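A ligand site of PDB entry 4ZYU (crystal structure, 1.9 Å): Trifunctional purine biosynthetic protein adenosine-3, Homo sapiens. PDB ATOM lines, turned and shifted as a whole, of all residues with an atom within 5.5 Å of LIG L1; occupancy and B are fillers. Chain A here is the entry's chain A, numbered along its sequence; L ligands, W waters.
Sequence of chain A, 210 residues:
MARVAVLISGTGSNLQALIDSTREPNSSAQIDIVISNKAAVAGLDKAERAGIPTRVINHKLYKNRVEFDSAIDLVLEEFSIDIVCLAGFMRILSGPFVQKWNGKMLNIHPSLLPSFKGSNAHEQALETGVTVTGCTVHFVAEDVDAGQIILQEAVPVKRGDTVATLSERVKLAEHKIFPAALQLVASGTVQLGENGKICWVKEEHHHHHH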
ATOM      1  N   HIS A  59      17.248  28.618 -14.275  1.00  0.00           N
ATOM      2  CA  HIS A  59      18.273  27.841 -13.573  1.00  0.00           C
ATOM      3  C   HIS A  59      19.142  28.656 -12.618  1.00  0.00           C
ATOM      4  O   HIS A  59      19.963  28.088 -11.893  1.00  0.00           O
ATOM      5  CB  HIS A  59      19.173  27.139 -14.589  1.00  0.00           C
ATOM      6  CG  HIS A  59      20.009  28.075 -15.407  1.00  0.00           C
ATOM      7  ND1 HIS A  59      19.498  28.749 -16.514  1.00  0.00           N
ATOM      8  CD2 HIS A  59      21.305  28.454 -15.311  1.00  0.00           C
ATOM      9  CE1 HIS A  59      20.447  29.493 -17.043  1.00  0.00           C
ATOM     10  NE2 HIS A  59      21.555  29.334 -16.340  1.00  0.00           N
ATOM     11  N   ARG A  65      22.447  21.894  -9.970  1.00  0.00           N
ATOM     12  CA  ARG A  65      21.874  21.315 -11.183  1.00  0.00           C
ATOM     13  C   ARG A  65      20.716  20.378 -10.876  1.00  0.00           C
ATOM     14  O   ARG A  65      19.698  20.387 -11.571  1.00  0.00           O
ATOM     15  CB  ARG A  65      22.965  20.566 -11.958  1.00  0.00           C
ATOM     16  CG  ARG A  65      22.512  19.971 -13.278  1.00  0.00           C
ATOM     17  CD  ARG A  65      23.709  19.679 -14.172  1.00  0.00           C
ATOM     18  NE  ARG A  65      24.484  20.883 -14.428  1.00  0.00           N
ATOM     19  CZ  ARG A  65      25.659  20.902 -15.065  1.00  0.00           C
ATOM     20  NH1 ARG A  65      26.196  19.782 -15.508  1.00  0.00           N
ATOM     21  NH2 ARG A  65      26.285  22.054 -15.249  1.00  0.00           N
ATOM     22  N   LEU A  86      14.458  18.097 -26.406  1.00  0.00           N
ATOM     23  CA  LEU A  86      15.314  19.266 -26.184  1.00  0.00           C
ATOM     24  C   LEU A  86      15.490  19.971 -27.525  1.00  0.00           C
ATOM     25  O   LEU A  86      16.067  19.392 -28.447  1.00  0.00           O
ATOM     26  CB  LEU A  86      16.667  18.864 -25.589  1.00  0.00           C
ATOM     27  CG  LEU A  86      16.633  17.976 -24.334  1.00  0.00           C
ATOM     28  CD1 LEU A  86      18.012  17.866 -23.710  1.00  0.00           C
ATOM     29  CD2 LEU A  86      15.603  18.459 -23.324  1.00  0.00           C
ATOM     30  N   PHE A  89      17.718  23.607 -26.357  1.00  0.00           N
ATOM     31  CA  PHE A  89      17.916  23.730 -24.907  1.00  0.00           C
ATOM     32  C   PHE A  89      19.413  23.635 -24.599  1.00  0.00           C
ATOM     33  O   PHE A  89      20.034  22.605 -24.834  1.00  0.00           O
ATOM     34  CB  PHE A  89      17.139  22.625 -24.173  1.00  0.00           C
ATOM     35  CG  PHE A  89      17.112  22.762 -22.661  1.00  0.00           C
ATOM     36  CD1 PHE A  89      16.247  23.656 -22.047  1.00  0.00           C
ATOM     37  CD2 PHE A  89      17.911  21.951 -21.864  1.00  0.00           C
ATOM     38  CE1 PHE A  89      16.190  23.759 -20.667  1.00  0.00           C
ATOM     39  CE2 PHE A  89      17.871  22.061 -20.470  1.00  0.00           C
ATOM     40  CZ  PHE A  89      16.999  22.956 -19.865  1.00  0.00           C
ATOM     41  N   MET A  90      19.989  24.720 -24.080  1.00  0.00           N
ATOM     42  CA  MET A  90      21.432  24.791 -23.907  1.00  0.00           C
ATOM     43  C   MET A  90      21.882  24.639 -22.445  1.00  0.00           C
ATOM     44  O   MET A  90      22.798  25.344 -22.016  1.00  0.00           O
ATOM     45  CB  MET A  90      21.985  26.109 -24.476  1.00  0.00           C
ATOM     46  CG  MET A  90      21.616  26.388 -25.927  1.00  0.00           C
ATOM     47  SD  MET A  90      22.195  25.147 -27.120  1.00  0.00           S
ATOM     48  CE  MET A  90      23.944  25.532 -27.182  1.00  0.00           C
ATOM     49  N   ARG A  91      21.243  23.739 -21.699  1.00  0.00           N
ATOM     50  CA  ARG A  91      21.690  23.396 -20.352  1.00  0.00           C
ATOM     51  C   ARG A  91      21.908  21.901 -20.163  1.00  0.00           C
ATOM     52  O   ARG A  91      21.026  21.099 -20.500  1.00  0.00           O
ATOM     53  CB  ARG A  91      20.683  23.881 -19.297  1.00  0.00           C
ATOM     54  CG  ARG A  91      20.507  25.376 -19.264  1.00  0.00           C
ATOM     55  CD  ARG A  91      20.484  25.870 -17.840  1.00  0.00           C
ATOM     56  NE  ARG A  91      21.808  25.856 -17.217  1.00  0.00           N
ATOM     57  CZ  ARG A  91      22.134  25.102 -16.164  1.00  0.00           C
ATOM     58  NH1 ARG A  91      21.237  24.300 -15.604  1.00  0.00           N
ATOM     59  NH2 ARG A  91      23.361  25.157 -15.674  1.00  0.00           N
ATOM     60  N   ILE A  92      23.049  21.515 -19.607  1.00  0.00           N
ATOM     61  CA  ILE A  92      23.337  20.102 -19.351  1.00  0.00           C
ATOM     62  C   ILE A  92      22.481  19.540 -18.209  1.00  0.00           C
ATOM     63  O   ILE A  92      22.374  20.154 -17.152  1.00  0.00           O
ATOM     64  CB  ILE A  92      24.827  19.891 -19.036  1.00  0.00           C
ATOM     65  CG1 ILE A  92      25.646  20.118 -20.305  1.00  0.00           C
ATOM     66  CG2 ILE A  92      25.080  18.503 -18.486  1.00  0.00           C
ATOM     67  CD1 ILE A  92      27.129  19.869 -20.127  1.00  0.00           C
ATOM     68  N   LEU A  93      21.855  18.386 -18.443  1.00  0.00           N
ATOM     69  CA  LEU A  93      20.959  17.768 -17.476  1.00  0.00           C
ATOM     70  C   LEU A  93      21.676  16.754 -16.569  1.00  0.00           C
ATOM     71  O   LEU A  93      22.607  16.075 -17.000  1.00  0.00           O
ATOM     72  CB  LEU A  93      19.813  17.074 -18.207  1.00  0.00           C
ATOM     73  CG  LEU A  93      18.904  18.023 -18.984  1.00  0.00           C
ATOM     74  CD1 LEU A  93      18.096  17.265 -20.044  1.00  0.00           C
ATOM     75  CD2 LEU A  93      17.968  18.728 -18.015  1.00  0.00           C
ATOM     76  N   SER A  94      21.211  16.642 -15.335  1.00  0.00           N
ATOM     77  CA  SER A  94      21.840  15.779 -14.336  1.00  0.00           C
ATOM     78  C   SER A  94      21.616  14.289 -14.578  1.00  0.00           C
ATOM     79  O   SER A  94      20.631  13.890 -15.219  1.00  0.00           O
ATOM     80  CB  SER A  94      21.320  16.126 -12.933  1.00  0.00           C
ATOM     81  OG  SER A  94      20.063  15.498 -12.688  1.00  0.00           O
ATOM     82  N   VAL A  98      18.341  12.359 -16.252  1.00  0.00           N
ATOM     83  CA  VAL A  98      18.549  11.664 -17.519  1.00  0.00           C
ATOM     84  C   VAL A  98      18.177  10.189 -17.381  1.00  0.00           C
ATOM     85  O   VAL A  98      17.520   9.619 -18.263  1.00  0.00           O
ATOM     86  CB  VAL A  98      20.013  11.805 -17.989  1.00  0.00           C
ATOM     87  CG1 VAL A  98      20.304  10.864 -19.151  1.00  0.00           C
ATOM     88  CG2 VAL A  98      20.299  13.245 -18.380  1.00  0.00           C
ATOM     89  N   ASN A 107      17.132  14.716 -28.327  1.00  0.00           N
ATOM     90  CA  ASN A 107      17.834  15.971 -28.536  1.00  0.00           C
ATOM     91  C   ASN A 107      18.227  16.111 -30.002  1.00  0.00           C
ATOM     92  O   ASN A 107      18.555  15.116 -30.641  1.00  0.00           O
ATOM     93  CB  ASN A 107      19.095  16.035 -27.654  1.00  0.00           C
ATOM     94  CG  ASN A 107      19.887  17.321 -27.866  1.00  0.00           C
ATOM     95  OD1 ASN A 107      19.361  18.425 -27.736  1.00  0.00           O
ATOM     96  ND2 ASN A 107      21.168  17.173 -28.194  1.00  0.00           N
ATOM     97  N   HIS A 109      21.040  17.845 -32.542  1.00  0.00           N
ATOM     98  CA  HIS A 109      22.399  18.362 -32.469  1.00  0.00           C
ATOM     99  C   HIS A 109      22.882  18.666 -33.878  1.00  0.00           C
ATOM    100  O   HIS A 109      22.718  17.838 -34.768  1.00  0.00           O
ATOM    101  CB  HIS A 109      23.311  17.354 -31.775  1.00  0.00           C
ATOM    102  CG  HIS A 109      24.723  17.815 -31.635  1.00  0.00           C
ATOM    103  ND1 HIS A 109      25.115  18.708 -30.661  1.00  0.00           N
ATOM    104  CD2 HIS A 109      25.834  17.549 -32.373  1.00  0.00           C
ATOM    105  CE1 HIS A 109      26.412  18.948 -30.792  1.00  0.00           C
ATOM    106  NE2 HIS A 109      26.865  18.245 -31.818  1.00  0.00           N
ATOM    107  N   GLY A 118      29.293  18.933 -28.445  1.00  0.00           N
ATOM    108  CA  GLY A 118      29.432  20.176 -27.703  1.00  0.00           C
ATOM    109  C   GLY A 118      28.560  21.304 -28.215  1.00  0.00           C
ATOM    110  O   GLY A 118      27.724  21.104 -29.093  1.00  0.00           O
ATOM    111  N   SER A 119      28.772  22.506 -27.684  1.00  0.00           N
ATOM    112  CA  SER A 119      27.836  23.599 -27.910  1.00  0.00           C
ATOM    113  C   SER A 119      28.135  24.451 -29.156  1.00  0.00           C
ATOM    114  O   SER A 119      27.304  25.302 -29.521  1.00  0.00           O
ATOM    115  CB  SER A 119      27.811  24.511 -26.689  1.00  0.00           C
ATOM    116  OG  SER A 119      29.053  25.168 -26.566  1.00  0.00           O
ATOM    117  N   HIS A 138      19.095  12.234 -31.347  1.00  0.00           N
ATOM    118  CA  HIS A 138      19.512  11.102 -30.547  1.00  0.00           C
ATOM    119  C   HIS A 138      18.781  11.073 -29.204  1.00  0.00           C
ATOM    120  O   HIS A 138      18.329  12.109 -28.719  1.00  0.00           O
ATOM    121  CB  HIS A 138      21.028  11.147 -30.295  1.00  0.00           C
ATOM    122  CG  HIS A 138      21.463  12.350 -29.504  1.00  0.00           C
ATOM    123  ND1 HIS A 138      21.638  12.318 -28.137  1.00  0.00           N
ATOM    124  CD2 HIS A 138      21.747  13.618 -29.896  1.00  0.00           C
ATOM    125  CE1 HIS A 138      22.022  13.508 -27.714  1.00  0.00           C
ATOM    126  NE2 HIS A 138      22.092  14.318 -28.763  1.00  0.00           N
ATOM    127  N   VAL A 140      18.839  11.083 -25.277  1.00  0.00           N
ATOM    128  CA  VAL A 140      19.753  11.718 -24.334  1.00  0.00           C
ATOM    129  C   VAL A 140      20.258  10.709 -23.302  1.00  0.00           C
ATOM    130  O   VAL A 140      19.473  10.063 -22.612  1.00  0.00           O
ATOM    131  CB  VAL A 140      19.074  12.899 -23.612  1.00  0.00           C
ATOM    132  CG1 VAL A 140      20.023  13.495 -22.586  1.00  0.00           C
ATOM    133  CG2 VAL A 140      18.631  13.939 -24.626  1.00  0.00           C
ATOM    134  N   ALA A 141      21.577  10.584 -23.227  1.00  0.00           N
ATOM    135  CA  ALA A 141      22.238   9.751 -22.224  1.00  0.00           C
ATOM    136  C   ALA A 141      23.033  10.673 -21.305  1.00  0.00           C
ATOM    137  O   ALA A 141      23.095  11.877 -21.544  1.00  0.00           O
ATOM    138  CB  ALA A 141      23.138   8.722 -22.876  1.00  0.00           C
ATOM    139  N   GLU A 142      23.623  10.128 -20.249  1.00  0.00           N
ATOM    140  CA  GLU A 142      24.276  10.968 -19.253  1.00  0.00           C
ATOM    141  C   GLU A 142      25.428  11.740 -19.898  1.00  0.00           C
ATOM    142  O   GLU A 142      25.561  12.949 -19.697  1.00  0.00           O
ATOM    143  CB  GLU A 142      24.763  10.143 -18.064  1.00  0.00           C
ATOM    144  CG  GLU A 142      24.993  10.990 -16.831  1.00  0.00           C
ATOM    145  CD  GLU A 142      25.584  10.208 -15.682  1.00  0.00           C
ATOM    146  OE1 GLU A 142      25.426   8.970 -15.650  1.00  0.00           O
ATOM    147  OE2 GLU A 142      26.201  10.840 -14.801  1.00  0.00           O
ATOM    148  N   ASP A 143      26.259  11.045 -20.658  1.00  0.00           N
ATOM    149  CA  ASP A 143      27.337  11.721 -21.381  1.00  0.00           C
ATOM    150  C   ASP A 143      26.796  12.506 -22.569  1.00  0.00           C
ATOM    151  O   ASP A 143      26.056  11.970 -23.397  1.00  0.00           O
ATOM    152  CB  ASP A 143      28.390  10.720 -21.844  1.00  0.00           C
ATOM    153  CG  ASP A 143      29.430  10.458 -20.782  1.00  0.00           C
ATOM    154  OD1 ASP A 143      29.602  11.324 -19.907  1.00  0.00           O
ATOM    155  OD2 ASP A 143      30.078   9.387 -20.826  1.00  0.00           O
ATOM    156  N   VAL A 144      27.176  13.777 -22.642  1.00  0.00           N
ATOM    157  CA  VAL A 144      26.615  14.726 -23.598  1.00  0.00           C
ATOM    158  C   VAL A 144      26.850  14.307 -25.065  1.00  0.00           C
ATOM    159  O   VAL A 144      27.967  13.958 -25.436  1.00  0.00           O
ATOM    160  CB  VAL A 144      27.201  16.132 -23.350  1.00  0.00           C
ATOM    161  CG1 VAL A 144      26.738  17.114 -24.417  1.00  0.00           C
ATOM    162  CG2 VAL A 144      26.800  16.630 -21.976  1.00  0.00           C
ATOM    163  N   ASP A 145      25.775  14.334 -25.867  1.00  0.00           N
ATOM    164  CA  ASP A 145      25.822  14.002 -27.309  1.00  0.00           C
ATOM    165  C   ASP A 145      26.383  12.608 -27.591  1.00  0.00           C
ATOM    166  O   ASP A 145      27.017  12.396 -28.628  1.00  0.00           O
ATOM    167  CB  ASP A 145      26.638  15.043 -28.079  1.00  0.00           C
ATOM    168  CG  ASP A 145      26.038  16.430 -28.007  1.00  0.00           C
ATOM    169  OD1 ASP A 145      24.796  16.544 -27.864  1.00  0.00           O
ATOM    170  OD2 ASP A 145      26.793  17.405 -28.089  1.00  0.00           O
ATOM    171  N   ALA A 146      26.146  11.675 -26.677  1.00  0.00           N
ATOM    172  CA  ALA A 146      26.686  10.315 -26.776  1.00  0.00           C
ATOM    173  C   ALA A 146      25.588   9.258 -26.777  1.00  0.00           C
ATOM    174  O   ALA A 146      25.867   8.068 -26.914  1.00  0.00           O
ATOM    175  CB  ALA A 146      27.688  10.050 -25.622  1.00  0.00           C
HETATM  176  C1  LIG L   1      27.082  21.931 -23.510  1.00  0.00           C
HETATM  177  C2  LIG L   1      25.219  23.466 -23.682  1.00  0.00           C
HETATM  178  C3  LIG L   1      24.702  22.710 -24.725  1.00  0.00           C
HETATM  179  N1  LIG L   1      22.454  16.658 -20.918  1.00  0.00           N
HETATM  180  C4  LIG L   1      22.946  15.413 -20.895  1.00  0.00           C
HETATM  181  N2  LIG L   1      23.209  14.728 -22.014  1.00  0.00           N
HETATM  182  C5  LIG L   1      23.016  15.247 -23.239  1.00  0.00           C
HETATM  183  S1  LIG L   1      21.644  18.688 -22.478  1.00  0.00           S
HETATM  184  C6  LIG L   1      21.738  18.527 -24.170  1.00  0.00           C
HETATM  185  C7  LIG L   1      22.220  17.276 -24.493  1.00  0.00           C
HETATM  186  C8  LIG L   1      22.507  16.527 -23.360  1.00  0.00           C
HETATM  187  C9  LIG L   1      22.264  17.149 -22.148  1.00  0.00           C
HETATM  188  O1  LIG L   1      23.289  14.559 -24.227  1.00  0.00           O
HETATM  189  N3  LIG L   1      23.190  14.786 -19.642  1.00  0.00           N
HETATM  190  C10 LIG L   1      26.409  23.079 -23.086  1.00  0.00           C
HETATM  191  C11 LIG L   1      26.974  23.915 -21.922  1.00  0.00           C
HETATM  192  O2  LIG L   1      27.436  25.017 -22.110  1.00  0.00           O
HETATM  193  N4  LIG L   1      26.931  23.335 -20.622  1.00  0.00           N
HETATM  194  C12 LIG L   1      27.404  24.031 -19.486  1.00  0.00           C
HETATM  195  C13 LIG L   1      26.361  23.912 -18.391  1.00  0.00           C
HETATM  196  C14 LIG L   1      25.065  24.480 -18.914  1.00  0.00           C
HETATM  197  C15 LIG L   1      25.327  25.892 -19.415  1.00  0.00           C
HETATM  198  O3  LIG L   1      25.203  26.172 -20.637  1.00  0.00           O
HETATM  199  O4  LIG L   1      25.686  26.777 -18.607  1.00  0.00           O
HETATM  200  C16 LIG L   1      28.757  23.528 -19.026  1.00  0.00           C
HETATM  201  O5  LIG L   1      28.923  22.299 -18.776  1.00  0.00           O
HETATM  202  O6  LIG L   1      29.720  24.324 -18.892  1.00  0.00           O
HETATM  203  C17 LIG L   1      21.321  19.605 -25.138  1.00  0.00           C
HETATM  204  C18 LIG L   1      22.481  20.551 -25.358  1.00  0.00           C
HETATM  205  C19 LIG L   1      23.678  19.789 -25.900  1.00  0.00           C
HETATM  206  C20 LIG L   1      24.793  20.740 -26.273  1.00  0.00           C
HETATM  207  C21 LIG L   1      25.375  21.571 -25.160  1.00  0.00           C
HETATM  208  C22 LIG L   1      26.554  21.172 -24.545  1.00  0.00           C
HETATM  209  C1  LG2 L   2      19.585  24.252 -33.279  1.00  0.00           C
HETATM  210  O1  LG2 L   2      20.315  24.455 -34.494  1.00  0.00           O
HETATM  211  C2  LG2 L   2      20.205  23.096 -32.537  1.00  0.00           C
HETATM  212  O2  LG2 L   2      20.748  22.147 -33.451  1.00  0.00           O
HETATM  213  C3  LG2 L   2      21.290  23.786 -31.721  1.00  0.00           C
HETATM  214  O3  LG2 L   2      20.694  25.033 -31.336  1.00  0.00           O
HETATM  215  C4  LG2 L   2      19.790  25.455 -32.376  1.00  0.00           C
HETATM  216  C5  LG2 L   2      18.468  25.948 -31.798  1.00  0.00           C
HETATM  217  O4  LG2 L   2      17.666  26.535 -32.826  1.00  0.00           O
HETATM  218  N1  LG2 L   2      21.708  22.998 -30.579  1.00  0.00           N
HETATM  219  C6  LG2 L   2      22.997  22.964 -30.220  1.00  0.00           C
HETATM  220  O5  LG2 L   2      23.877  23.556 -30.835  1.00  0.00           O
HETATM  221  C7  LG2 L   2      23.329  22.134 -29.001  1.00  0.00           C
HETATM  222  N2  LG2 L   2      22.572  20.897 -28.990  1.00  0.00           N
HETATM  223  P1  LG2 L   2      16.107  26.844 -32.588  1.00  0.00           P
HETATM  224  O6  LG2 L   2      15.727  27.720 -33.765  1.00  0.00           O
HETATM  225  O7  LG2 L   2      16.040  27.547 -31.239  1.00  0.00           O
HETATM  226  O8  LG2 L   2      15.468  25.478 -32.563  1.00  0.00           O
HETATM  227  O   HOH W   1      18.969  20.982 -27.121  1.00  0.00           O
HETATM  228  O   HOH W   2      23.634  11.894 -24.777  1.00  0.00           O
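O of Arg 91 sits close to S1 of LIG L1. Merely in contact with LIG L1: Phe 89 (3.2 Å), Ile 92 (3.3 Å), Val 144 (3.4 Å), Asn 107 (3.5 Å), Val 140 (3.5 Å), Val 98 (3.5 Å), Arg 65 (3.7 Å), Leu 86 (3.8 Å), His 138 (3.9 Å) and Asp 143 (3.9 Å). Of the 22 residues printed, 16 come within 4 Å of LIG L1.
The side-chain carboxylate of Asp 145 lies close to a ring nitrogen (ND1) of His 109, 3.3 Å away. The side-chain carboxylate of Asp 145 sits at hydrogen-bond distance from the backbone NH of Gly 118, at 3.0 Å. N of Asn 107 lies within hydrogen-bond range of O of His 138, at 2.9 Å.
An oxygen (O1) of LIG L1 lies within hydrogen-bond range of the backbone NH (N) of Asp 145. A nitrogen (N3) of LIG L1 lies within hydrogen-bond range of the backbone carbonyl oxygen (O) of Ala 141. The backbone carbonyl oxygen (O) of Leu 93 lies within hydrogen-bond range of a nitrogen (N3) of LIG L1 (3.0 Å). The backbone carbonyl oxygen (O) of Met 90 lies close to an oxygen (O3) of LIG L1 (2.9 Å). A nitrogen (N3) of LIG L1 lies within hydrogen-bond range of the backbone carbonyl oxygen of Glu 142.
Water W1 lies within hydrogen-bond range of OD1 of Asn 107 and O of Phe 89.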
